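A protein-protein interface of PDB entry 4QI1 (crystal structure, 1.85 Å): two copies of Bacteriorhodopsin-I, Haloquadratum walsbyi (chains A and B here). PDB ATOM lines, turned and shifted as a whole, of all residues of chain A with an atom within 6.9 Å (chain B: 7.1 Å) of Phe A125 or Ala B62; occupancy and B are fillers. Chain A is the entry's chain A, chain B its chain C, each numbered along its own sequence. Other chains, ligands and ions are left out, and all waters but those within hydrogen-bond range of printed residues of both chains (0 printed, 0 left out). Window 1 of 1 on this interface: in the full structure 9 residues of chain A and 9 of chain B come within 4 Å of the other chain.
Of the printed residues of chain B, Phe A125 touches Ala B58 and Ala B62. Ala B62 touches just these residues of chain A: Phe A125 and Phe A145. Printed residues of chain A within 4 Å of Leu B65: Phe A145 (3.97 Å) and Ile A148 (3.6 Å). Of the printed residues of chain B, Ile A148 touches Leu B65. Of the printed residues of chain A, Ala B58 touches Phe A125 (3.5 Å). Of the printed residues of chain B, Phe A145 touches Ala B62, Leu B65 and Ser B66. The nearest printed residue of chain B that does not touch Phe A125 is Ile B59 (4.01 Å). The nearest printed residue of chain A that does not touch Ala B58 is Thr A129 (6.6 Å).
Hydrophobic or aromatic side chains of chain B within 4 Å of the printed part of chain A: Ala B62 and Leu B65. Of the 19 printed residues of chain A, 3 touch a printed residue of chain B. Hydrophobic or aromatic side chains of chain A within 4 Å of the printed part of chain B: Phe A125, Phe A145 and Ile A148. Among the printed residues, 6 pairs touch across the chains.
Among the printed residues, pairs that only touch across the chains: Phe A145 with Ala B62, Phe A125 with Ala B58, Ile A148 with Leu B65, Phe A145 with Ser B66, Phe A145 with Leu B65 and Phe A125 with Ala B62.
No position is printed for both chains. Of the 6 pairs that touch across the chains among the printed residues, none has its exchanged pair printed and touching as well.
The backbone carbonyl oxygen of Phe A125 lies within hydrogen-bond range of the side-chain hydroxyl of Thr A129, at 2.8 Å. OG1 of Thr B24 lies within hydrogen-bond range of N of Leu B65 (3.3 Å). O of Ser B63 lies within hydrogen-bond range of OG of Ser B66 (2.8 Å).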
ATOM      1  N   LEU A  95      17.211 -27.853  17.924  1.00  0.00           N
ATOM      2  CA  LEU A  95      17.511 -26.491  18.336  1.00  0.00           C
ATOM      3  C   LEU A  95      18.859 -26.005  17.852  1.00  0.00           C
ATOM      4  O   LEU A  95      19.031 -24.818  17.606  1.00  0.00           O
ATOM      5  CB  LEU A  95      17.427 -26.317  19.850  1.00  0.00           C
ATOM      6  CG  LEU A  95      17.324 -24.863  20.283  1.00  0.00           C
ATOM      7  CD1 LEU A  95      16.020 -24.252  19.734  1.00  0.00           C
ATOM      8  CD2 LEU A  95      17.381 -24.821  21.819  1.00  0.00           C
ATOM      9  N   LEU A 119      16.617 -15.519  10.065  1.00  0.00           N
ATOM     10  CA  LEU A 119      16.088 -16.825   9.828  1.00  0.00           C
ATOM     11  C   LEU A 119      16.300 -17.672  11.041  1.00  0.00           C
ATOM     12  O   LEU A 119      15.412 -18.469  11.384  1.00  0.00           O
ATOM     13  CB  LEU A 119      16.641 -17.544   8.573  1.00  0.00           C
ATOM     14  CG  LEU A 119      15.992 -17.183   7.247  1.00  0.00           C
ATOM     15  CD1 LEU A 119      16.455 -18.061   6.081  1.00  0.00           C
ATOM     16  CD2 LEU A 119      14.507 -17.338   7.422  1.00  0.00           C
ATOM     17  N   VAL A 120      17.477 -17.570  11.659  1.00  0.00           N
ATOM     18  CA  VAL A 120      17.795 -18.353  12.831  1.00  0.00           C
ATOM     19  C   VAL A 120      16.815 -18.092  14.011  1.00  0.00           C
ATOM     20  O   VAL A 120      16.357 -19.014  14.674  1.00  0.00           O
ATOM     21  CB  VAL A 120      19.239 -18.161  13.245  1.00  0.00           C
ATOM     22  CG1 VAL A 120      19.455 -18.659  14.673  1.00  0.00           C
ATOM     23  CG2 VAL A 120      20.161 -18.898  12.266  1.00  0.00           C
ATOM     24  N   GLY A 121      16.483 -16.817  14.216  1.00  0.00           N
ATOM     25  CA  GLY A 121      15.479 -16.430  15.208  1.00  0.00           C
ATOM     26  C   GLY A 121      14.124 -17.084  14.992  1.00  0.00           C
ATOM     27  O   GLY A 121      13.496 -17.616  15.977  1.00  0.00           O
ATOM     28  N   ILE A 122      13.679 -17.069  13.735  1.00  0.00           N
ATOM     29  CA  ILE A 122      12.390 -17.658  13.332  1.00  0.00           C
ATOM     30  C   ILE A 122      12.482 -19.179  13.506  1.00  0.00           C
ATOM     31  O   ILE A 122      11.545 -19.804  13.975  1.00  0.00           O
ATOM     32  CB  ILE A 122      12.061 -17.355  11.868  1.00  0.00           C
ATOM     33  CG1 ILE A 122      11.913 -15.852  11.698  1.00  0.00           C
ATOM     34  CG2 ILE A 122      10.786 -18.064  11.421  1.00  0.00           C
ATOM     35  CD1 ILE A 122      11.698 -15.491  10.241  1.00  0.00           C
ATOM     36  N   ASP A 123      13.643 -19.722  13.139  1.00  0.00           N
ATOM     37  CA  ASP A 123      13.903 -21.139  13.296  1.00  0.00           C
ATOM     38  C   ASP A 123      13.816 -21.609  14.741  1.00  0.00           C
ATOM     39  O   ASP A 123      13.116 -22.629  15.034  1.00  0.00           O
ATOM     40  CB  ASP A 123      15.217 -21.531  12.720  1.00  0.00           C
ATOM     41  CG  ASP A 123      15.493 -23.049  12.832  1.00  0.00           C
ATOM     42  OD1 ASP A 123      15.117 -23.791  11.922  1.00  0.00           O
ATOM     43  OD2 ASP A 123      16.139 -23.452  13.766  1.00  0.00           O
ATOM     44  N   ALA A 124      14.554 -20.934  15.629  1.00  0.00           N
ATOM     45  CA  ALA A 124      14.456 -21.209  17.087  1.00  0.00           C
ATOM     46  C   ALA A 124      13.002 -21.160  17.573  1.00  0.00           C
ATOM     47  O   ALA A 124      12.589 -22.019  18.324  1.00  0.00           O
ATOM     48  CB  ALA A 124      15.272 -20.172  17.843  1.00  0.00           C
ATOM     49  N   PHE A 125      12.277 -20.100  17.202  1.00  0.00           N
ATOM     50  CA  PHE A 125      10.843 -19.975  17.528  1.00  0.00           C
ATOM     51  C   PHE A 125      10.090 -21.205  17.059  1.00  0.00           C
ATOM     52  O   PHE A 125       9.263 -21.790  17.876  1.00  0.00           O
ATOM     53  CB  PHE A 125      10.250 -18.767  16.829  1.00  0.00           C
ATOM     54  CG  PHE A 125       8.811 -18.453  17.238  1.00  0.00           C
ATOM     55  CD1 PHE A 125       7.764 -18.944  16.490  1.00  0.00           C
ATOM     56  CD2 PHE A 125       8.535 -17.714  18.317  1.00  0.00           C
ATOM     57  CE1 PHE A 125       6.429 -18.675  16.848  1.00  0.00           C
ATOM     58  CE2 PHE A 125       7.201 -17.463  18.736  1.00  0.00           C
ATOM     59  CZ  PHE A 125       6.162 -17.892  17.966  1.00  0.00           C
ATOM     60  N   MET A 126      10.351 -21.634  15.800  1.00  0.00           N
ATOM     61  CA  MET A 126       9.708 -22.852  15.266  1.00  0.00           C
ATOM     62  C   MET A 126       9.932 -24.116  16.131  1.00  0.00           C
ATOM     63  O   MET A 126       8.992 -24.872  16.544  1.00  0.00           O
ATOM     64  CB  MET A 126      10.127 -23.064  13.840  1.00  0.00           C
ATOM     65  CG  MET A 126       9.568 -24.321  13.198  1.00  0.00           C
ATOM     66  SD  MET A 126      10.288 -24.664  11.570  1.00  0.00           S
ATOM     67  CE  MET A 126      11.952 -25.181  12.055  1.00  0.00           C
ATOM     68  N   ILE A 127      11.170 -24.368  16.501  1.00  0.00           N
ATOM     69  CA  ILE A 127      11.488 -25.520  17.333  1.00  0.00           C
ATOM     70  C   ILE A 127      10.951 -25.480  18.788  1.00  0.00           C
ATOM     71  O   ILE A 127      10.406 -26.436  19.322  1.00  0.00           O
ATOM     72  CB  ILE A 127      13.047 -25.788  17.351  1.00  0.00           C
ATOM     73  CG1 ILE A 127      13.613 -25.986  15.961  1.00  0.00           C
ATOM     74  CG2 ILE A 127      13.391 -26.924  18.292  1.00  0.00           C
ATOM     75  CD1 ILE A 127      12.944 -27.065  15.053  1.00  0.00           C
ATOM     76  N   VAL A 128      11.093 -24.360  19.465  1.00  0.00           N
ATOM     77  CA  VAL A 128      10.583 -24.251  20.789  1.00  0.00           C
ATOM     78  C   VAL A 128       9.057 -24.359  20.858  1.00  0.00           C
ATOM     79  O   VAL A 128       8.530 -25.044  21.754  1.00  0.00           O
ATOM     80  CB  VAL A 128      11.103 -22.960  21.471  1.00  0.00           C
ATOM     81  CG1 VAL A 128      10.651 -22.941  22.892  1.00  0.00           C
ATOM     82  CG2 VAL A 128      12.612 -22.947  21.398  1.00  0.00           C
ATOM     83  N   THR A 129       8.339 -23.721  19.931  1.00  0.00           N
ATOM     84  CA  THR A 129       6.873 -23.809  19.945  1.00  0.00           C
ATOM     85  C   THR A 129       6.429 -25.223  19.597  1.00  0.00           C
ATOM     86  O   THR A 129       5.443 -25.692  20.170  1.00  0.00           O
ATOM     87  CB  THR A 129       6.165 -22.795  19.088  1.00  0.00           C
ATOM     88  OG1 THR A 129       6.684 -22.858  17.714  1.00  0.00           O
ATOM     89  CG2 THR A 129       6.316 -21.404  19.743  1.00  0.00           C
ATOM     90  N   GLY A 130       7.226 -25.936  18.786  1.00  0.00           N
ATOM     91  CA  GLY A 130       7.112 -27.395  18.626  1.00  0.00           C
ATOM     92  C   GLY A 130       7.295 -28.222  19.874  1.00  0.00           C
ATOM     93  O   GLY A 130       6.569 -29.180  20.058  1.00  0.00           O
ATOM     94  N   LEU A 131       8.275 -27.868  20.712  1.00  0.00           N
ATOM     95  CA  LEU A 131       8.539 -28.599  21.911  1.00  0.00           C
ATOM     96  C   LEU A 131       7.357 -28.400  22.900  1.00  0.00           C
ATOM     97  O   LEU A 131       6.940 -29.365  23.514  1.00  0.00           O
ATOM     98  CB  LEU A 131       9.820 -28.120  22.547  1.00  0.00           C
ATOM     99  CG  LEU A 131      10.199 -28.752  23.886  1.00  0.00           C
ATOM    100  CD1 LEU A 131      10.401 -30.257  23.780  1.00  0.00           C
ATOM    101  CD2 LEU A 131      11.449 -28.068  24.429  1.00  0.00           C
ATOM    102  N   VAL A 132       6.830 -27.156  23.029  1.00  0.00           N
ATOM    103  CA  VAL A 132       5.585 -26.913  23.772  1.00  0.00           C
ATOM    104  C   VAL A 132       4.401 -27.786  23.286  1.00  0.00           C
ATOM    105  O   VAL A 132       3.722 -28.452  24.099  1.00  0.00           O
ATOM    106  CB  VAL A 132       5.178 -25.438  23.762  1.00  0.00           C
ATOM    107  CG1 VAL A 132       3.904 -25.258  24.527  1.00  0.00           C
ATOM    108  CG2 VAL A 132       6.292 -24.611  24.396  1.00  0.00           C
ATOM    109  N   PHE A 145      -0.249 -25.043  19.296  1.00  0.00           N
ATOM    110  CA  PHE A 145       1.194 -24.871  19.195  1.00  0.00           C
ATOM    111  C   PHE A 145       1.788 -25.519  17.953  1.00  0.00           C
ATOM    112  O   PHE A 145       2.750 -25.016  17.385  1.00  0.00           O
ATOM    113  CB  PHE A 145       1.945 -25.252  20.482  1.00  0.00           C
ATOM    114  CG  PHE A 145       1.981 -24.160  21.468  1.00  0.00           C
ATOM    115  CD1 PHE A 145       2.948 -23.191  21.455  1.00  0.00           C
ATOM    116  CD2 PHE A 145       0.925 -24.033  22.354  1.00  0.00           C
ATOM    117  CE1 PHE A 145       2.937 -22.154  22.402  1.00  0.00           C
ATOM    118  CE2 PHE A 145       0.919 -23.069  23.321  1.00  0.00           C
ATOM    119  CZ  PHE A 145       1.868 -22.071  23.289  1.00  0.00           C
ATOM    120  N   ILE A 148       0.966 -22.821  15.425  1.00  0.00           N
ATOM    121  CA  ILE A 148       1.949 -21.748  15.571  1.00  0.00           C
ATOM    122  C   ILE A 148       3.310 -22.126  14.980  1.00  0.00           C
ATOM    123  O   ILE A 148       3.861 -21.391  14.201  1.00  0.00           O
ATOM    124  CB  ILE A 148       2.104 -21.339  17.027  1.00  0.00           C
ATOM    125  CG1 ILE A 148       0.825 -20.595  17.465  1.00  0.00           C
ATOM    126  CG2 ILE A 148       3.365 -20.450  17.262  1.00  0.00           C
ATOM    127  CD1 ILE A 148       0.539 -20.663  18.956  1.00  0.00           C
ATOM    128  N   SER A 149       3.797 -23.307  15.316  1.00  0.00           N
ATOM    129  CA  SER A 149       5.104 -23.753  14.828  1.00  0.00           C
ATOM    130  C   SER A 149       5.101 -23.928  13.283  1.00  0.00           C
ATOM    131  O   SER A 149       6.035 -23.434  12.528  1.00  0.00           O
ATOM    132  CB  SER A 149       5.493 -25.042  15.529  1.00  0.00           C
ATOM    133  OG  SER A 149       6.759 -25.444  15.067  1.00  0.00           O
ATOM    134  N   SER A 152       5.218 -20.586  11.469  1.00  0.00           N
ATOM    135  CA  SER A 152       6.550 -20.090  11.520  1.00  0.00           C
ATOM    136  C   SER A 152       7.498 -20.821  10.502  1.00  0.00           C
ATOM    137  O   SER A 152       8.309 -20.209   9.877  1.00  0.00           O
ATOM    138  CB  SER A 152       7.073 -20.088  12.983  1.00  0.00           C
ATOM    139  OG  SER A 152       7.399 -21.387  13.371  1.00  0.00           O
ATOM    140  N   THR B  24      -1.580 -12.379  26.106  1.00  0.00           N
ATOM    141  CA  THR B  24      -1.537 -13.037  24.762  1.00  0.00           C
ATOM    142  C   THR B  24      -2.067 -12.174  23.676  1.00  0.00           C
ATOM    143  O   THR B  24      -1.351 -11.896  22.690  1.00  0.00           O
ATOM    144  CB  THR B  24      -2.261 -14.414  24.711  1.00  0.00           C
ATOM    145  OG1 THR B  24      -1.824 -15.192  25.811  1.00  0.00           O
ATOM    146  CG2 THR B  24      -1.967 -15.128  23.404  1.00  0.00           C
ATOM    147  N   MET B  27      -0.016  -8.719  23.103  1.00  0.00           N
ATOM    148  CA  MET B  27       1.261  -9.072  22.414  1.00  0.00           C
ATOM    149  C   MET B  27       1.045  -9.449  20.944  1.00  0.00           C
ATOM    150  O   MET B  27       1.714  -8.943  20.008  1.00  0.00           O
ATOM    151  CB  MET B  27       1.975 -10.240  23.074  1.00  0.00           C
ATOM    152  CG  MET B  27       2.533  -9.983  24.446  1.00  0.00           C
ATOM    153  SD  MET B  27       3.793  -8.673  24.464  1.00  0.00           S
ATOM    154  CE  MET B  27       3.977  -8.745  26.241  1.00  0.00           C
ATOM    155  N   MET B  31       2.396  -7.404  17.676  1.00  0.00           N
ATOM    156  CA  MET B  31       3.136  -8.140  16.621  1.00  0.00           C
ATOM    157  C   MET B  31       2.491  -7.901  15.239  1.00  0.00           C
ATOM    158  O   MET B  31       3.191  -7.530  14.267  1.00  0.00           O
ATOM    159  CB  MET B  31       3.252  -9.625  16.957  1.00  0.00           C
ATOM    160  CG  MET B  31       4.082 -10.416  15.951  1.00  0.00           C
ATOM    161  SD  MET B  31       3.729 -12.144  16.067  1.00  0.00           S
ATOM    162  CE  MET B  31       2.169 -12.280  15.263  1.00  0.00           C
ATOM    163  N   LEU B  55       9.818 -10.077  16.486  1.00  0.00           N
ATOM    164  CA  LEU B  55      10.195 -11.352  17.223  1.00  0.00           C
ATOM    165  C   LEU B  55       9.958 -11.300  18.722  1.00  0.00           C
ATOM    166  O   LEU B  55       9.604 -12.322  19.379  1.00  0.00           O
ATOM    167  CB  LEU B  55      11.667 -11.682  16.986  1.00  0.00           C
ATOM    168  CG  LEU B  55      12.169 -13.062  16.583  1.00  0.00           C
ATOM    169  CD1 LEU B  55      13.577 -13.218  17.229  1.00  0.00           C
ATOM    170  CD2 LEU B  55      11.283 -14.244  16.893  1.00  0.00           C
ATOM    171  N   ILE B  56      10.156 -10.114  19.294  1.00  0.00           N
ATOM    172  CA  ILE B  56       9.925  -9.889  20.746  1.00  0.00           C
ATOM    173  C   ILE B  56       8.482 -10.190  21.252  1.00  0.00           C
ATOM    174  O   ILE B  56       8.274 -11.110  22.098  1.00  0.00           O
ATOM    175  CB  ILE B  56      10.454  -8.491  21.181  1.00  0.00           C
ATOM    176  CG1 ILE B  56      11.966  -8.389  21.066  1.00  0.00           C
ATOM    177  CG2 ILE B  56       9.998  -8.176  22.606  1.00  0.00           C
ATOM    178  CD1 ILE B  56      12.447  -6.948  20.951  1.00  0.00           C
ATOM    179  N   PRO B  57       7.478  -9.544  20.659  1.00  0.00           N
ATOM    180  CA  PRO B  57       6.129  -9.935  21.083  1.00  0.00           C
ATOM    181  C   PRO B  57       5.622 -11.270  20.525  1.00  0.00           C
ATOM    182  O   PRO B  57       4.724 -11.859  21.154  1.00  0.00           O
ATOM    183  CB  PRO B  57       5.231  -8.793  20.593  1.00  0.00           C
ATOM    184  CG  PRO B  57       5.978  -8.133  19.538  1.00  0.00           C
ATOM    185  CD  PRO B  57       7.441  -8.327  19.765  1.00  0.00           C
ATOM    186  N   ALA B  58       6.134 -11.726  19.408  1.00  0.00           N
ATOM    187  CA  ALA B  58       5.936 -13.141  19.027  1.00  0.00           C
ATOM    188  C   ALA B  58       6.304 -14.116  20.138  1.00  0.00           C
ATOM    189  O   ALA B  58       5.462 -14.946  20.535  1.00  0.00           O
ATOM    190  CB  ALA B  58       6.680 -13.456  17.744  1.00  0.00           C
ATOM    191  N   ILE B  59       7.518 -13.979  20.686  1.00  0.00           N
ATOM    192  CA  ILE B  59       8.028 -14.866  21.738  1.00  0.00           C
ATOM    193  C   ILE B  59       7.102 -14.691  22.979  1.00  0.00           C
ATOM    194  O   ILE B  59       6.594 -15.664  23.556  1.00  0.00           O
ATOM    195  CB  ILE B  59       9.521 -14.551  22.041  1.00  0.00           C
ATOM    196  CG1 ILE B  59      10.428 -15.063  20.912  1.00  0.00           C
ATOM    197  CG2 ILE B  59       9.951 -15.147  23.384  1.00  0.00           C
ATOM    198  CD1 ILE B  59      11.706 -14.301  20.821  1.00  0.00           C
ATOM    199  N   ALA B  60       6.800 -13.448  23.320  1.00  0.00           N
ATOM    200  CA  ALA B  60       5.989 -13.148  24.483  1.00  0.00           C
ATOM    201  C   ALA B  60       4.556 -13.599  24.337  1.00  0.00           C
ATOM    202  O   ALA B  60       4.041 -14.165  25.275  1.00  0.00           O
ATOM    203  CB  ALA B  60       6.080 -11.674  24.844  1.00  0.00           C
ATOM    204  N   ALA B  61       3.966 -13.464  23.147  1.00  0.00           N
ATOM    205  CA  ALA B  61       2.601 -13.970  22.927  1.00  0.00           C
ATOM    206  C   ALA B  61       2.597 -15.514  23.129  1.00  0.00           C
ATOM    207  O   ALA B  61       1.745 -16.067  23.766  1.00  0.00           O
ATOM    208  CB  ALA B  61       2.109 -13.630  21.518  1.00  0.00           C
ATOM    209  N   ALA B  62       3.586 -16.221  22.570  1.00  0.00           N
ATOM    210  CA  ALA B  62       3.655 -17.674  22.701  1.00  0.00           C
ATOM    211  C   ALA B  62       3.847 -18.131  24.157  1.00  0.00           C
ATOM    212  O   ALA B  62       3.204 -19.125  24.588  1.00  0.00           O
ATOM    213  CB  ALA B  62       4.759 -18.228  21.771  1.00  0.00           C
ATOM    214  N   SER B  63       4.681 -17.403  24.911  1.00  0.00           N
ATOM    215  CA  SER B  63       4.918 -17.685  26.328  1.00  0.00           C
ATOM    216  C   SER B  63       3.640 -17.465  27.174  1.00  0.00           C
ATOM    217  O   SER B  63       3.219 -18.376  27.901  1.00  0.00           O
ATOM    218  CB  SER B  63       6.060 -16.813  26.859  1.00  0.00           C
ATOM    219  OG  SER B  63       6.191 -17.059  28.228  1.00  0.00           O
ATOM    220  N   TYR B  64       2.971 -16.320  26.970  1.00  0.00           N
ATOM    221  CA  TYR B  64       1.642 -16.086  27.547  1.00  0.00           C
ATOM    222  C   TYR B  64       0.595 -17.167  27.227  1.00  0.00           C
ATOM    223  O   TYR B  64      -0.177 -17.597  28.075  1.00  0.00           O
ATOM    224  CB  TYR B  64       1.124 -14.656  27.153  1.00  0.00           C
ATOM    225  CG  TYR B  64       1.644 -13.610  28.148  1.00  0.00           C
ATOM    226  CD1 TYR B  64       2.939 -13.099  28.062  1.00  0.00           C
ATOM    227  CD2 TYR B  64       0.870 -13.242  29.264  1.00  0.00           C
ATOM    228  CE1 TYR B  64       3.426 -12.212  29.070  1.00  0.00           C
ATOM    229  CE2 TYR B  64       1.370 -12.396  30.275  1.00  0.00           C
ATOM    230  CZ  TYR B  64       2.637 -11.858  30.164  1.00  0.00           C
ATOM    231  OH  TYR B  64       3.089 -11.001  31.147  1.00  0.00           O
ATOM    232  N   LEU B  65       0.488 -17.531  25.977  1.00  0.00           N
ATOM    233  CA  LEU B  65      -0.494 -18.592  25.594  1.00  0.00           C
ATOM    234  C   LEU B  65      -0.153 -19.904  26.291  1.00  0.00           C
ATOM    235  O   LEU B  65      -1.063 -20.656  26.696  1.00  0.00           O
ATOM    236  CB  LEU B  65      -0.484 -18.752  24.114  1.00  0.00           C
ATOM    237  CG  LEU B  65      -1.485 -19.744  23.523  1.00  0.00           C
ATOM    238  CD1 LEU B  65      -2.896 -19.250  23.727  1.00  0.00           C
ATOM    239  CD2 LEU B  65      -1.207 -19.899  22.044  1.00  0.00           C
ATOM    240  N   SER B  66       1.161 -20.245  26.365  1.00  0.00           N
ATOM    241  CA  SER B  66       1.610 -21.461  27.002  1.00  0.00           C
ATOM    242  C   SER B  66       1.205 -21.417  28.494  1.00  0.00           C
ATOM    243  O   SER B  66       0.607 -22.420  28.966  1.00  0.00           O
ATOM    244  CB  SER B  66       3.103 -21.774  26.778  1.00  0.00           C
ATOM    245  OG  SER B  66       3.952 -21.057  27.617  1.00  0.00           O
ATOM    246  N   MET B  67       1.400 -20.249  29.163  1.00  0.00           N
ATOM    247  CA  MET B  67       1.008 -20.111  30.557  1.00  0.00           C
ATOM    248  C   MET B  67      -0.538 -20.202  30.681  1.00  0.00           C
ATOM    249  O   MET B  67      -1.014 -20.888  31.570  1.00  0.00           O
ATOM    250  CB  MET B  67       1.562 -18.857  31.194  1.00  0.00           C
ATOM    251  CG  MET B  67       3.065 -18.821  31.225  1.00  0.00           C
ATOM    252  SD  MET B  67       3.774 -17.394  32.057  1.00  0.00           S
ATOM    253  CE  MET B  67       3.846 -16.195  30.734  1.00  0.00           C
ATOM    254  N   PHE B  68      -1.285 -19.637  29.735  1.00  0.00           N
ATOM    255  CA  PHE B  68      -2.759 -19.634  29.841  1.00  0.00           C
ATOM    256  C   PHE B  68      -3.225 -21.105  29.876  1.00  0.00           C
ATOM    257  O   PHE B  68      -4.123 -21.486  30.593  1.00  0.00           O
ATOM    258  CB  PHE B  68      -3.312 -18.902  28.630  1.00  0.00           C
ATOM    259  CG  PHE B  68      -4.787 -19.048  28.471  1.00  0.00           C
ATOM    260  CD1 PHE B  68      -5.647 -18.307  29.289  1.00  0.00           C
ATOM    261  CD2 PHE B  68      -5.312 -19.978  27.596  1.00  0.00           C
ATOM    262  CE1 PHE B  68      -7.022 -18.450  29.219  1.00  0.00           C
ATOM    263  CE2 PHE B  68      -6.713 -20.134  27.516  1.00  0.00           C
ATOM    264  CZ  PHE B  68      -7.562 -19.335  28.312  1.00  0.00           C
ATOM    265  N   ALA B  89       7.676 -20.283  32.751  1.00  0.00           N
ATOM    266  CA  ALA B  89       7.725 -19.963  31.320  1.00  0.00           C
ATOM    267  C   ALA B  89       8.077 -18.491  31.065  1.00  0.00           C
ATOM    268  O   ALA B  89       8.642 -18.159  30.008  1.00  0.00           O
ATOM    269  CB  ALA B  89       6.409 -20.344  30.661  1.00  0.00           C
ATOM    270  N   ASP B  93      10.831 -16.827  28.283  1.00  0.00           N
ATOM    271  CA  ASP B  93      10.500 -15.634  27.506  1.00  0.00           C
ATOM    272  C   ASP B  93      11.576 -14.558  27.727  1.00  0.00           C
ATOM    273  O   ASP B  93      12.186 -14.090  26.774  1.00  0.00           O
ATOM    274  CB  ASP B  93       9.081 -15.136  27.920  1.00  0.00           C
ATOM    275  CG  ASP B  93       8.697 -13.695  27.385  1.00  0.00           C
ATOM    276  OD1 ASP B  93       9.543 -12.927  26.859  1.00  0.00           O
ATOM    277  OD2 ASP B  93       7.499 -13.304  27.537  1.00  0.00           O
